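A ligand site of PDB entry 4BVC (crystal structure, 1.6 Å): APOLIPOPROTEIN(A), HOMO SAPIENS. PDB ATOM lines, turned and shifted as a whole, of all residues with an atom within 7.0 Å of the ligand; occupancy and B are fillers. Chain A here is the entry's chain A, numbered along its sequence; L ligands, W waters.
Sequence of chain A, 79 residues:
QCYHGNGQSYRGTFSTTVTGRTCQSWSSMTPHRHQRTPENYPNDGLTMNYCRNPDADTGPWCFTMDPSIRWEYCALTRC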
ATOM      1  N   ARG A  33       3.549   0.470   2.683  1.00  0.00           N
ATOM      2  CA  ARG A  33       2.408   0.315   1.791  1.00  0.00           C
ATOM      3  C   ARG A  33       2.851   0.754   0.412  1.00  0.00           C
ATOM      4  O   ARG A  33       3.459   1.811   0.246  1.00  0.00           O
ATOM      5  CB  ARG A  33       1.189   1.119   2.262  1.00  0.00           C
ATOM      6  CG  ARG A  33      -0.068   0.895   1.438  1.00  0.00           C
ATOM      7  CD  ARG A  33      -1.340   1.348   2.167  1.00  0.00           C
ATOM      8  NE  ARG A  33      -1.559   0.563   3.373  1.00  0.00           N
ATOM      9  CZ  ARG A  33      -2.172  -0.624   3.439  1.00  0.00           C
ATOM     10  NH1 ARG A  33      -2.690  -1.213   2.349  1.00  0.00           N
ATOM     11  NH2 ARG A  33      -2.284  -1.229   4.620  1.00  0.00           N
ATOM     12  N   HIS A  34       2.544  -0.063  -0.587  1.00  0.00           N
ATOM     13  CA  HIS A  34       3.002   0.172  -1.939  1.00  0.00           C
ATOM     14  C   HIS A  34       2.092  -0.556  -2.917  1.00  0.00           C
ATOM     15  O   HIS A  34       1.190  -1.278  -2.503  1.00  0.00           O
ATOM     16  CB  HIS A  34       4.433  -0.346  -2.084  1.00  0.00           C
ATOM     17  CG  HIS A  34       4.536  -1.836  -1.985  1.00  0.00           C
ATOM     18  ND1 HIS A  34       4.492  -2.656  -3.082  1.00  0.00           N
ATOM     19  CD2 HIS A  34       4.633  -2.652  -0.908  1.00  0.00           C
ATOM     20  CE1 HIS A  34       4.590  -3.910  -2.702  1.00  0.00           C
ATOM     21  NE2 HIS A  34       4.666  -3.947  -1.382  1.00  0.00           N
ATOM     22  N   GLN A  35       2.363  -0.369  -4.196  1.00  0.00           N
ATOM     23  CA  GLN A  35       1.526  -0.900  -5.255  1.00  0.00           C
ATOM     24  C   GLN A  35       2.237  -1.944  -6.094  1.00  0.00           C
ATOM     25  O   GLN A  35       1.673  -2.504  -7.007  1.00  0.00           O
ATOM     26  CB  GLN A  35       1.045   0.231  -6.164  1.00  0.00           C
ATOM     27  CG  GLN A  35       0.072   1.168  -5.466  1.00  0.00           C
ATOM     28  CD  GLN A  35      -0.203   2.398  -6.264  1.00  0.00           C
ATOM     29  OE1 GLN A  35      -0.865   2.351  -7.285  1.00  0.00           O
ATOM     30  NE2 GLN A  35       0.321   3.529  -5.806  1.00  0.00           N
ATOM     31  N   ARG A  36       3.513  -2.165  -5.810  1.00  0.00           N
ATOM     32  CA  ARG A  36       4.327  -3.047  -6.623  1.00  0.00           C
ATOM     33  C   ARG A  36       4.172  -4.492  -6.166  1.00  0.00           C
ATOM     34  O   ARG A  36       5.109  -5.117  -5.701  1.00  0.00           O
ATOM     35  CB  ARG A  36       5.785  -2.595  -6.570  1.00  0.00           C
ATOM     36  CG  ARG A  36       6.711  -3.364  -7.475  1.00  0.00           C
ATOM     37  CD  ARG A  36       6.343  -3.159  -8.937  1.00  0.00           C
ATOM     38  NE  ARG A  36       6.561  -1.799  -9.382  1.00  0.00           N
ATOM     39  CZ  ARG A  36       6.445  -1.419 -10.651  1.00  0.00           C
ATOM     40  NH1 ARG A  36       6.107  -2.312 -11.560  1.00  0.00           N
ATOM     41  NH2 ARG A  36       6.659  -0.168 -11.002  1.00  0.00           N
ATOM     42  N   THR A  37       2.961  -5.004  -6.296  1.00  0.00           N
ATOM     43  CA  THR A  37       2.653  -6.348  -5.870  1.00  0.00           C
ATOM     44  C   THR A  37       2.604  -7.353  -7.013  1.00  0.00           C
ATOM     45  O   THR A  37       2.421  -7.016  -8.136  1.00  0.00           O
ATOM     46  CB  THR A  37       1.287  -6.385  -5.172  1.00  0.00           C
ATOM     47  OG1 THR A  37       0.292  -6.034  -6.126  1.00  0.00           O
ATOM     48  CG2 THR A  37       1.268  -5.439  -4.010  1.00  0.00           C
ATOM     49  N   ASN A  40      -0.604  -7.143  -9.003  1.00  0.00           N
ATOM     50  CA  ASN A  40      -0.622  -5.981  -9.868  1.00  0.00           C
ATOM     51  C   ASN A  40       0.354  -6.121 -11.017  1.00  0.00           C
ATOM     52  O   ASN A  40       0.127  -5.593 -12.074  1.00  0.00           O
ATOM     53  CB  ASN A  40      -0.341  -4.665  -9.093  1.00  0.00           C
ATOM     54  CG  ASN A  40      -1.473  -4.270  -8.156  1.00  0.00           C
ATOM     55  OD1 ASN A  40      -2.585  -4.732  -8.286  1.00  0.00           O
ATOM     56  ND2 ASN A  40      -1.169  -3.385  -7.217  1.00  0.00           N
ATOM     57  N   TYR A  41       1.442  -6.859 -10.787  1.00  0.00           N
ATOM     58  CA  TYR A  41       2.543  -7.015 -11.735  1.00  0.00           C
ATOM     59  C   TYR A  41       2.942  -8.486 -11.896  1.00  0.00           C
ATOM     60  O   TYR A  41       3.990  -8.910 -11.389  1.00  0.00           O
ATOM     61  CB  TYR A  41       3.719  -6.139 -11.267  1.00  0.00           C
ATOM     62  CG  TYR A  41       3.341  -4.671 -11.303  1.00  0.00           C
ATOM     63  CD1 TYR A  41       3.333  -3.981 -12.511  1.00  0.00           C
ATOM     64  CD2 TYR A  41       2.937  -4.002 -10.156  1.00  0.00           C
ATOM     65  CE1 TYR A  41       2.965  -2.654 -12.571  1.00  0.00           C
ATOM     66  CE2 TYR A  41       2.554  -2.665 -10.204  1.00  0.00           C
ATOM     67  CZ  TYR A  41       2.570  -1.994 -11.412  1.00  0.00           C
ATOM     68  OH  TYR A  41       2.206  -0.662 -11.480  1.00  0.00           O
ATOM     69  N   ASN A  53      13.940  -5.923 -10.253  1.00  0.00           N
ATOM     70  CA  ASN A  53      13.853  -4.619 -10.902  1.00  0.00           C
ATOM     71  C   ASN A  53      12.659  -4.565 -11.848  1.00  0.00           C
ATOM     72  O   ASN A  53      12.835  -4.731 -13.055  1.00  0.00           O
ATOM     73  CB  ASN A  53      15.168  -4.302 -11.633  1.00  0.00           C
ATOM     74  CG  ASN A  53      15.133  -2.934 -12.320  1.00  0.00           C
ATOM     75  OD1 ASN A  53      14.260  -2.102 -12.054  1.00  0.00           O
ATOM     76  ND2 ASN A  53      16.094  -2.702 -13.194  1.00  0.00           N
ATOM     77  N   PRO A  54      11.451  -4.344 -11.305  1.00  0.00           N
ATOM     78  CA  PRO A  54      10.286  -4.354 -12.176  1.00  0.00           C
ATOM     79  C   PRO A  54      10.012  -3.029 -12.900  1.00  0.00           C
ATOM     80  O   PRO A  54       9.108  -2.978 -13.738  1.00  0.00           O
ATOM     81  CB  PRO A  54       9.137  -4.641 -11.207  1.00  0.00           C
ATOM     82  CG  PRO A  54       9.577  -4.008  -9.946  1.00  0.00           C
ATOM     83  CD  PRO A  54      11.048  -4.259  -9.885  1.00  0.00           C
ATOM     84  N   ASP A  55      10.766  -1.976 -12.590  1.00  0.00           N
ATOM     85  CA  ASP A  55      10.458  -0.639 -13.091  1.00  0.00           C
ATOM     86  C   ASP A  55      11.612   0.003 -13.850  1.00  0.00           C
ATOM     87  O   ASP A  55      11.688   1.230 -13.949  1.00  0.00           O
ATOM     88  CB  ASP A  55       9.978   0.257 -11.945  1.00  0.00           C
ATOM     89  CG  ASP A  55      11.054   0.525 -10.908  1.00  0.00           C
ATOM     90  OD1 ASP A  55      12.075  -0.189 -10.885  1.00  0.00           O
ATOM     91  OD2 ASP A  55      10.871   1.466 -10.107  1.00  0.00           O
ATOM     92  N   ALA A  56      12.487  -0.829 -14.410  1.00  0.00           N
ATOM     93  CA  ALA A  56      13.581  -0.342 -15.236  1.00  0.00           C
ATOM     94  C   ALA A  56      14.437   0.684 -14.485  1.00  0.00           C
ATOM     95  O   ALA A  56      14.842   1.713 -15.034  1.00  0.00           O
ATOM     96  CB  ALA A  56      13.044   0.229 -16.537  1.00  0.00           C
ATOM     97  N   ASP A  57      14.714   0.377 -13.222  1.00  0.00           N
ATOM     98  CA  ASP A  57      15.740   1.088 -12.496  1.00  0.00           C
ATOM     99  C   ASP A  57      17.065   0.530 -12.999  1.00  0.00           C
ATOM    100  O   ASP A  57      17.100  -0.104 -14.039  1.00  0.00           O
ATOM    101  CB  ASP A  57      15.553   0.943 -10.971  1.00  0.00           C
ATOM    102  CG  ASP A  57      16.131   2.111 -10.193  1.00  0.00           C
ATOM    103  OD1 ASP A  57      17.288   2.429 -10.419  1.00  0.00           O
ATOM    104  OD2 ASP A  57      15.435   2.674  -9.353  1.00  0.00           O
ATOM    105  N   THR A  58      18.147   0.766 -12.275  1.00  0.00           N
ATOM    106  CA  THR A  58      19.438   0.393 -12.788  1.00  0.00           C
ATOM    107  C   THR A  58      20.089  -0.773 -12.067  1.00  0.00           C
ATOM    108  O   THR A  58      21.185  -1.152 -12.368  1.00  0.00           O
ATOM    109  CB  THR A  58      20.358   1.604 -12.888  1.00  0.00           C
ATOM    110  OG1 THR A  58      20.408   2.238 -11.628  1.00  0.00           O
ATOM    111  CG2 THR A  58      19.803   2.561 -13.919  1.00  0.00           C
ATOM    112  N   TRP A  61      16.304  -4.125  -6.701  1.00  0.00           N
ATOM    113  CA  TRP A  61      16.064  -3.368  -5.470  1.00  0.00           C
ATOM    114  C   TRP A  61      14.900  -4.038  -4.732  1.00  0.00           C
ATOM    115  O   TRP A  61      14.361  -5.013  -5.186  1.00  0.00           O
ATOM    116  CB  TRP A  61      15.699  -1.910  -5.790  1.00  0.00           C
ATOM    117  CG  TRP A  61      14.512  -1.750  -6.727  1.00  0.00           C
ATOM    118  CD1 TRP A  61      14.541  -1.725  -8.082  1.00  0.00           C
ATOM    119  CD2 TRP A  61      13.145  -1.598  -6.355  1.00  0.00           C
ATOM    120  NE1 TRP A  61      13.264  -1.570  -8.578  1.00  0.00           N
ATOM    121  CE2 TRP A  61      12.390  -1.489  -7.534  1.00  0.00           C
ATOM    122  CE3 TRP A  61      12.477  -1.539  -5.139  1.00  0.00           C
ATOM    123  CZ2 TRP A  61      11.005  -1.337  -7.517  1.00  0.00           C
ATOM    124  CZ3 TRP A  61      11.128  -1.398  -5.125  1.00  0.00           C
ATOM    125  CH2 TRP A  61      10.402  -1.291  -6.305  1.00  0.00           C
ATOM    126  N   CYS A  62      14.568  -3.499  -3.572  1.00  0.00           N
ATOM    127  CA  CYS A  62      13.392  -3.942  -2.846  1.00  0.00           C
ATOM    128  C   CYS A  62      12.973  -2.892  -1.841  1.00  0.00           C
ATOM    129  O   CYS A  62      13.768  -2.015  -1.486  1.00  0.00           O
ATOM    130  CB  CYS A  62      13.683  -5.236  -2.094  1.00  0.00           C
ATOM    131  SG  CYS A  62      15.052  -5.094  -0.926  1.00  0.00           S
ATOM    132  N   PHE A  63      11.718  -2.962  -1.395  1.00  0.00           N
ATOM    133  CA  PHE A  63      11.300  -2.236  -0.216  1.00  0.00           C
ATOM    134  C   PHE A  63      11.989  -2.880   0.979  1.00  0.00           C
ATOM    135  O   PHE A  63      12.216  -4.086   0.964  1.00  0.00           O
ATOM    136  CB  PHE A  63       9.796  -2.287  -0.041  1.00  0.00           C
ATOM    137  CG  PHE A  63       9.063  -1.702  -1.195  1.00  0.00           C
ATOM    138  CD1 PHE A  63       8.932  -0.330  -1.320  1.00  0.00           C
ATOM    139  CD2 PHE A  63       8.500  -2.515  -2.170  1.00  0.00           C
ATOM    140  CE1 PHE A  63       8.267   0.221  -2.399  1.00  0.00           C
ATOM    141  CE2 PHE A  63       7.826  -1.962  -3.239  1.00  0.00           C
ATOM    142  CZ  PHE A  63       7.710  -0.606  -3.355  1.00  0.00           C
ATOM    143  N   ARG A  70      12.278   3.395   2.759  1.00  0.00           N
ATOM    144  CA  ARG A  70      11.261   2.780   1.907  1.00  0.00           C
ATOM    145  C   ARG A  70      11.830   1.709   0.971  1.00  0.00           C
ATOM    146  O   ARG A  70      11.302   0.602   0.898  1.00  0.00           O
ATOM    147  CB  ARG A  70      10.517   3.837   1.097  1.00  0.00           C
ATOM    148  CG  ARG A  70       9.395   3.272   0.241  1.00  0.00           C
ATOM    149  CD  ARG A  70       8.579   4.376  -0.392  1.00  0.00           C
ATOM    150  NE  ARG A  70       7.496   3.829  -1.205  1.00  0.00           N
ATOM    151  CZ  ARG A  70       6.339   3.374  -0.735  1.00  0.00           C
ATOM    152  NH1 ARG A  70       6.070   3.379   0.555  1.00  0.00           N
ATOM    153  NH2 ARG A  70       5.437   2.912  -1.587  1.00  0.00           N
ATOM    154  N   TRP A  71      12.899   2.039   0.262  1.00  0.00           N
ATOM    155  CA  TRP A  71      13.512   1.074  -0.661  1.00  0.00           C
ATOM    156  C   TRP A  71      15.002   1.334  -0.834  1.00  0.00           C
ATOM    157  O   TRP A  71      15.478   2.434  -0.572  1.00  0.00           O
ATOM    158  CB  TRP A  71      12.805   1.107  -2.022  1.00  0.00           C
ATOM    159  CG  TRP A  71      13.094   2.350  -2.805  1.00  0.00           C
ATOM    160  CD1 TRP A  71      12.442   3.548  -2.723  1.00  0.00           C
ATOM    161  CD2 TRP A  71      14.132   2.526  -3.771  1.00  0.00           C
ATOM    162  NE1 TRP A  71      13.017   4.461  -3.577  1.00  0.00           N
ATOM    163  CE2 TRP A  71      14.052   3.860  -4.244  1.00  0.00           C
ATOM    164  CE3 TRP A  71      15.124   1.682  -4.297  1.00  0.00           C
ATOM    165  CZ2 TRP A  71      14.923   4.362  -5.215  1.00  0.00           C
ATOM    166  CZ3 TRP A  71      15.985   2.186  -5.258  1.00  0.00           C
ATOM    167  CH2 TRP A  71      15.876   3.517  -5.708  1.00  0.00           C
ATOM    168  N   GLU A  72      15.711   0.295  -1.260  1.00  0.00           N
ATOM    169  CA  GLU A  72      17.128   0.387  -1.578  1.00  0.00           C
ATOM    170  C   GLU A  72      17.512  -0.584  -2.676  1.00  0.00           C
ATOM    171  O   GLU A  72      16.835  -1.596  -2.884  1.00  0.00           O
ATOM    172  CB  GLU A  72      17.953   0.009  -0.362  1.00  0.00           C
ATOM    173  CG  GLU A  72      17.911   0.961   0.807  1.00  0.00           C
ATOM    174  CD  GLU A  72      18.796   0.465   1.922  1.00  0.00           C
ATOM    175  OE1 GLU A  72      18.397  -0.497   2.607  1.00  0.00           O
ATOM    176  OE2 GLU A  72      19.898   0.990   2.075  1.00  0.00           O
ATOM    177  N   TYR A  73      18.634  -0.308  -3.331  1.00  0.00           N
ATOM    178  CA  TYR A  73      19.254  -1.281  -4.205  1.00  0.00           C
ATOM    179  C   TYR A  73      19.781  -2.437  -3.355  1.00  0.00           C
ATOM    180  O   TYR A  73      20.176  -2.246  -2.199  1.00  0.00           O
ATOM    181  CB  TYR A  73      20.406  -0.679  -5.005  1.00  0.00           C
ATOM    182  CG  TYR A  73      19.965   0.393  -5.959  1.00  0.00           C
ATOM    183  CD1 TYR A  73      19.293   0.074  -7.136  1.00  0.00           C
ATOM    184  CD2 TYR A  73      20.232   1.736  -5.699  1.00  0.00           C
ATOM    185  CE1 TYR A  73      18.882   1.058  -8.019  1.00  0.00           C
ATOM    186  CE2 TYR A  73      19.836   2.727  -6.571  1.00  0.00           C
ATOM    187  CZ  TYR A  73      19.169   2.394  -7.728  1.00  0.00           C
ATOM    188  OH  TYR A  73      18.775   3.408  -8.583  1.00  0.00           O
HETATM  189  C1  LIG L   1       3.554   5.569  -7.875  1.00  0.00           C
HETATM  190  C2  LIG L   1       3.555   5.679  -6.506  1.00  0.00           C
HETATM  191  C3  LIG L   1       3.952   4.612  -5.723  1.00  0.00           C
HETATM  192  C4  LIG L   1       4.336   3.450  -6.356  1.00  0.00           C
HETATM  193  C5  LIG L   1       4.330   3.323  -7.725  1.00  0.00           C
HETATM  194  C6  LIG L   1       3.940   4.395  -8.502  1.00  0.00           C
HETATM  195  O1  LIG L   1       4.742   2.116  -8.259  1.00  0.00           O
HETATM  196  C7  LIG L   1       3.780   1.479  -9.113  1.00  0.00           C
HETATM  197  F1  LIG L   1       2.486   1.608  -8.696  1.00  0.00           F
HETATM  198  F2  LIG L   1       4.077   0.138  -9.145  1.00  0.00           F
HETATM  199  F3  LIG L   1       3.908   1.991 -10.373  1.00  0.00           F
HETATM  200  S1  LIG L   1       4.837   2.059  -5.390  1.00  0.00           S
HETATM  201  O2  LIG L   1       4.262   0.881  -5.994  1.00  0.00           O
HETATM  202  O3  LIG L   1       4.525   2.364  -4.001  1.00  0.00           O
HETATM  203  N1  LIG L   1       6.521   2.083  -5.666  1.00  0.00           N
HETATM  204  C8  LIG L   1       7.404   2.810  -4.842  1.00  0.00           C
HETATM  205  O4  LIG L   1       7.027   3.548  -3.944  1.00  0.00           O
HETATM  206  C9  LIG L   1       8.847   2.568  -5.147  1.00  0.00           C
HETATM  207  C10 LIG L   1       9.281   3.575  -6.197  1.00  0.00           C
HETATM  208  C11 LIG L   1      10.773   3.524  -6.496  1.00  0.00           C
HETATM  209  C12 LIG L   1      11.313   2.101  -6.586  1.00  0.00           C
HETATM  210  C13 LIG L   1      12.699   2.045  -7.181  1.00  0.00           C
HETATM  211  N2  LIG L   1      12.694   2.658  -8.514  1.00  0.00           N
HETATM  212  C14 LIG L   1      12.380   4.072  -8.338  1.00  0.00           C
HETATM  213  C15 LIG L   1      10.976   4.238  -7.808  1.00  0.00           C
HETATM  214  O   HOH W   1      -0.368   2.883  -9.925  1.00  0.00           O
HETATM  215  O   HOH W   2       7.494   0.218  -7.549  1.00  0.00           O
HETATM  216  O   HOH W   3       3.037   0.740 -13.447  1.00  0.00           O
HETATM  217  O   HOH W   4       3.424   3.486 -13.162  1.00  0.00           O
HETATM  218  O   HOH W   5       1.788   3.584  -3.570  1.00  0.00           O
HETATM  219  O   HOH W   6       0.178   5.910  -7.958  1.00  0.00           O
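O2 of the ligand sits at hydrogen-bond distance from N of Gln 35 (2.9 Å).
The guanidinium group (NH2) of Arg 70 sits at hydrogen-bond distance from an oxygen (O3) of the ligand.
The side-chain carboxylate (OD2) of Asp 55 lies within salt-bridge range of a nitrogen (N2) of the ligand (2.7 Å).
An oxygen (O2) of the ligand lies within hydrogen-bond range of the backbone NH (N) of Arg 36 (3.1 Å).
N2 of the ligand lies within salt-bridge range of OD2 of Asp 57, 2.9 Å away.
NH2 of Arg 70 sits at hydrogen-bond distance from O of Arg 33, 2.9 Å away.
The side-chain carboxylate of Asp 55 lies within hydrogen-bond range of the indole nitrogen of Trp 61 (2.9 Å).
OD1 of Asn 53 lies close to OD1 of Asp 55 (3.1 Å).
The backbone NH (N) of Asp 57 sits at hydrogen-bond distance from the side-chain amide oxygen (OD1) of Asn 53 (2.8 Å).
The side-chain hydroxyl (OG1) of Thr 58 sits at hydrogen-bond distance from the side-chain carboxylate (OD1) of Asp 57 (3.4 Å).
The backbone NH of Arg 36 sits at hydrogen-bond distance from a ring nitrogen (ND1) of His 34 (2.9 Å).
The side-chain carboxylate of Asp 57 is in hydrogen-bond range of the side-chain hydroxyl of Tyr 73.
The backbone carbonyl oxygen (O) of Gln 35 is in hydrogen-bond range of the side-chain amide nitrogen (ND2) of Asn 40 (3.0 Å).
The side-chain hydroxyl (OH) of Tyr 41 lies close to a fluorine (F2) of the ligand (3.1 Å).
His 34 touches the ligand (CB to O3, 3.3 Å).
Trp 61 touches the ligand (CH2 to C12, 3.5 Å).
Phe 63 touches the ligand.
Trp 71 touches the ligand.
Hydrophobic or aromatic side chains within 4 Å of the ligand: His 34, Tyr 41, Trp 61, Phe 63 and Trp 71.
Of the 20 residues printed, 10 come within 4 Å of the ligand.
Along chain A the residues within 4 Å of the ligand span positions 34 to 71.
The nearest printed residue that does not touch the ligand is Arg 33 (4.4 Å).
Water W2 bridges a nitrogen (N1) of the ligand (2.8 Å) and the guanidinium group of Arg 36 (2.9 Å).
Water W5 lies within hydrogen-bond range of NE2 of Gln 35 (2.7 Å) and O3 of the ligand (3.0 Å).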
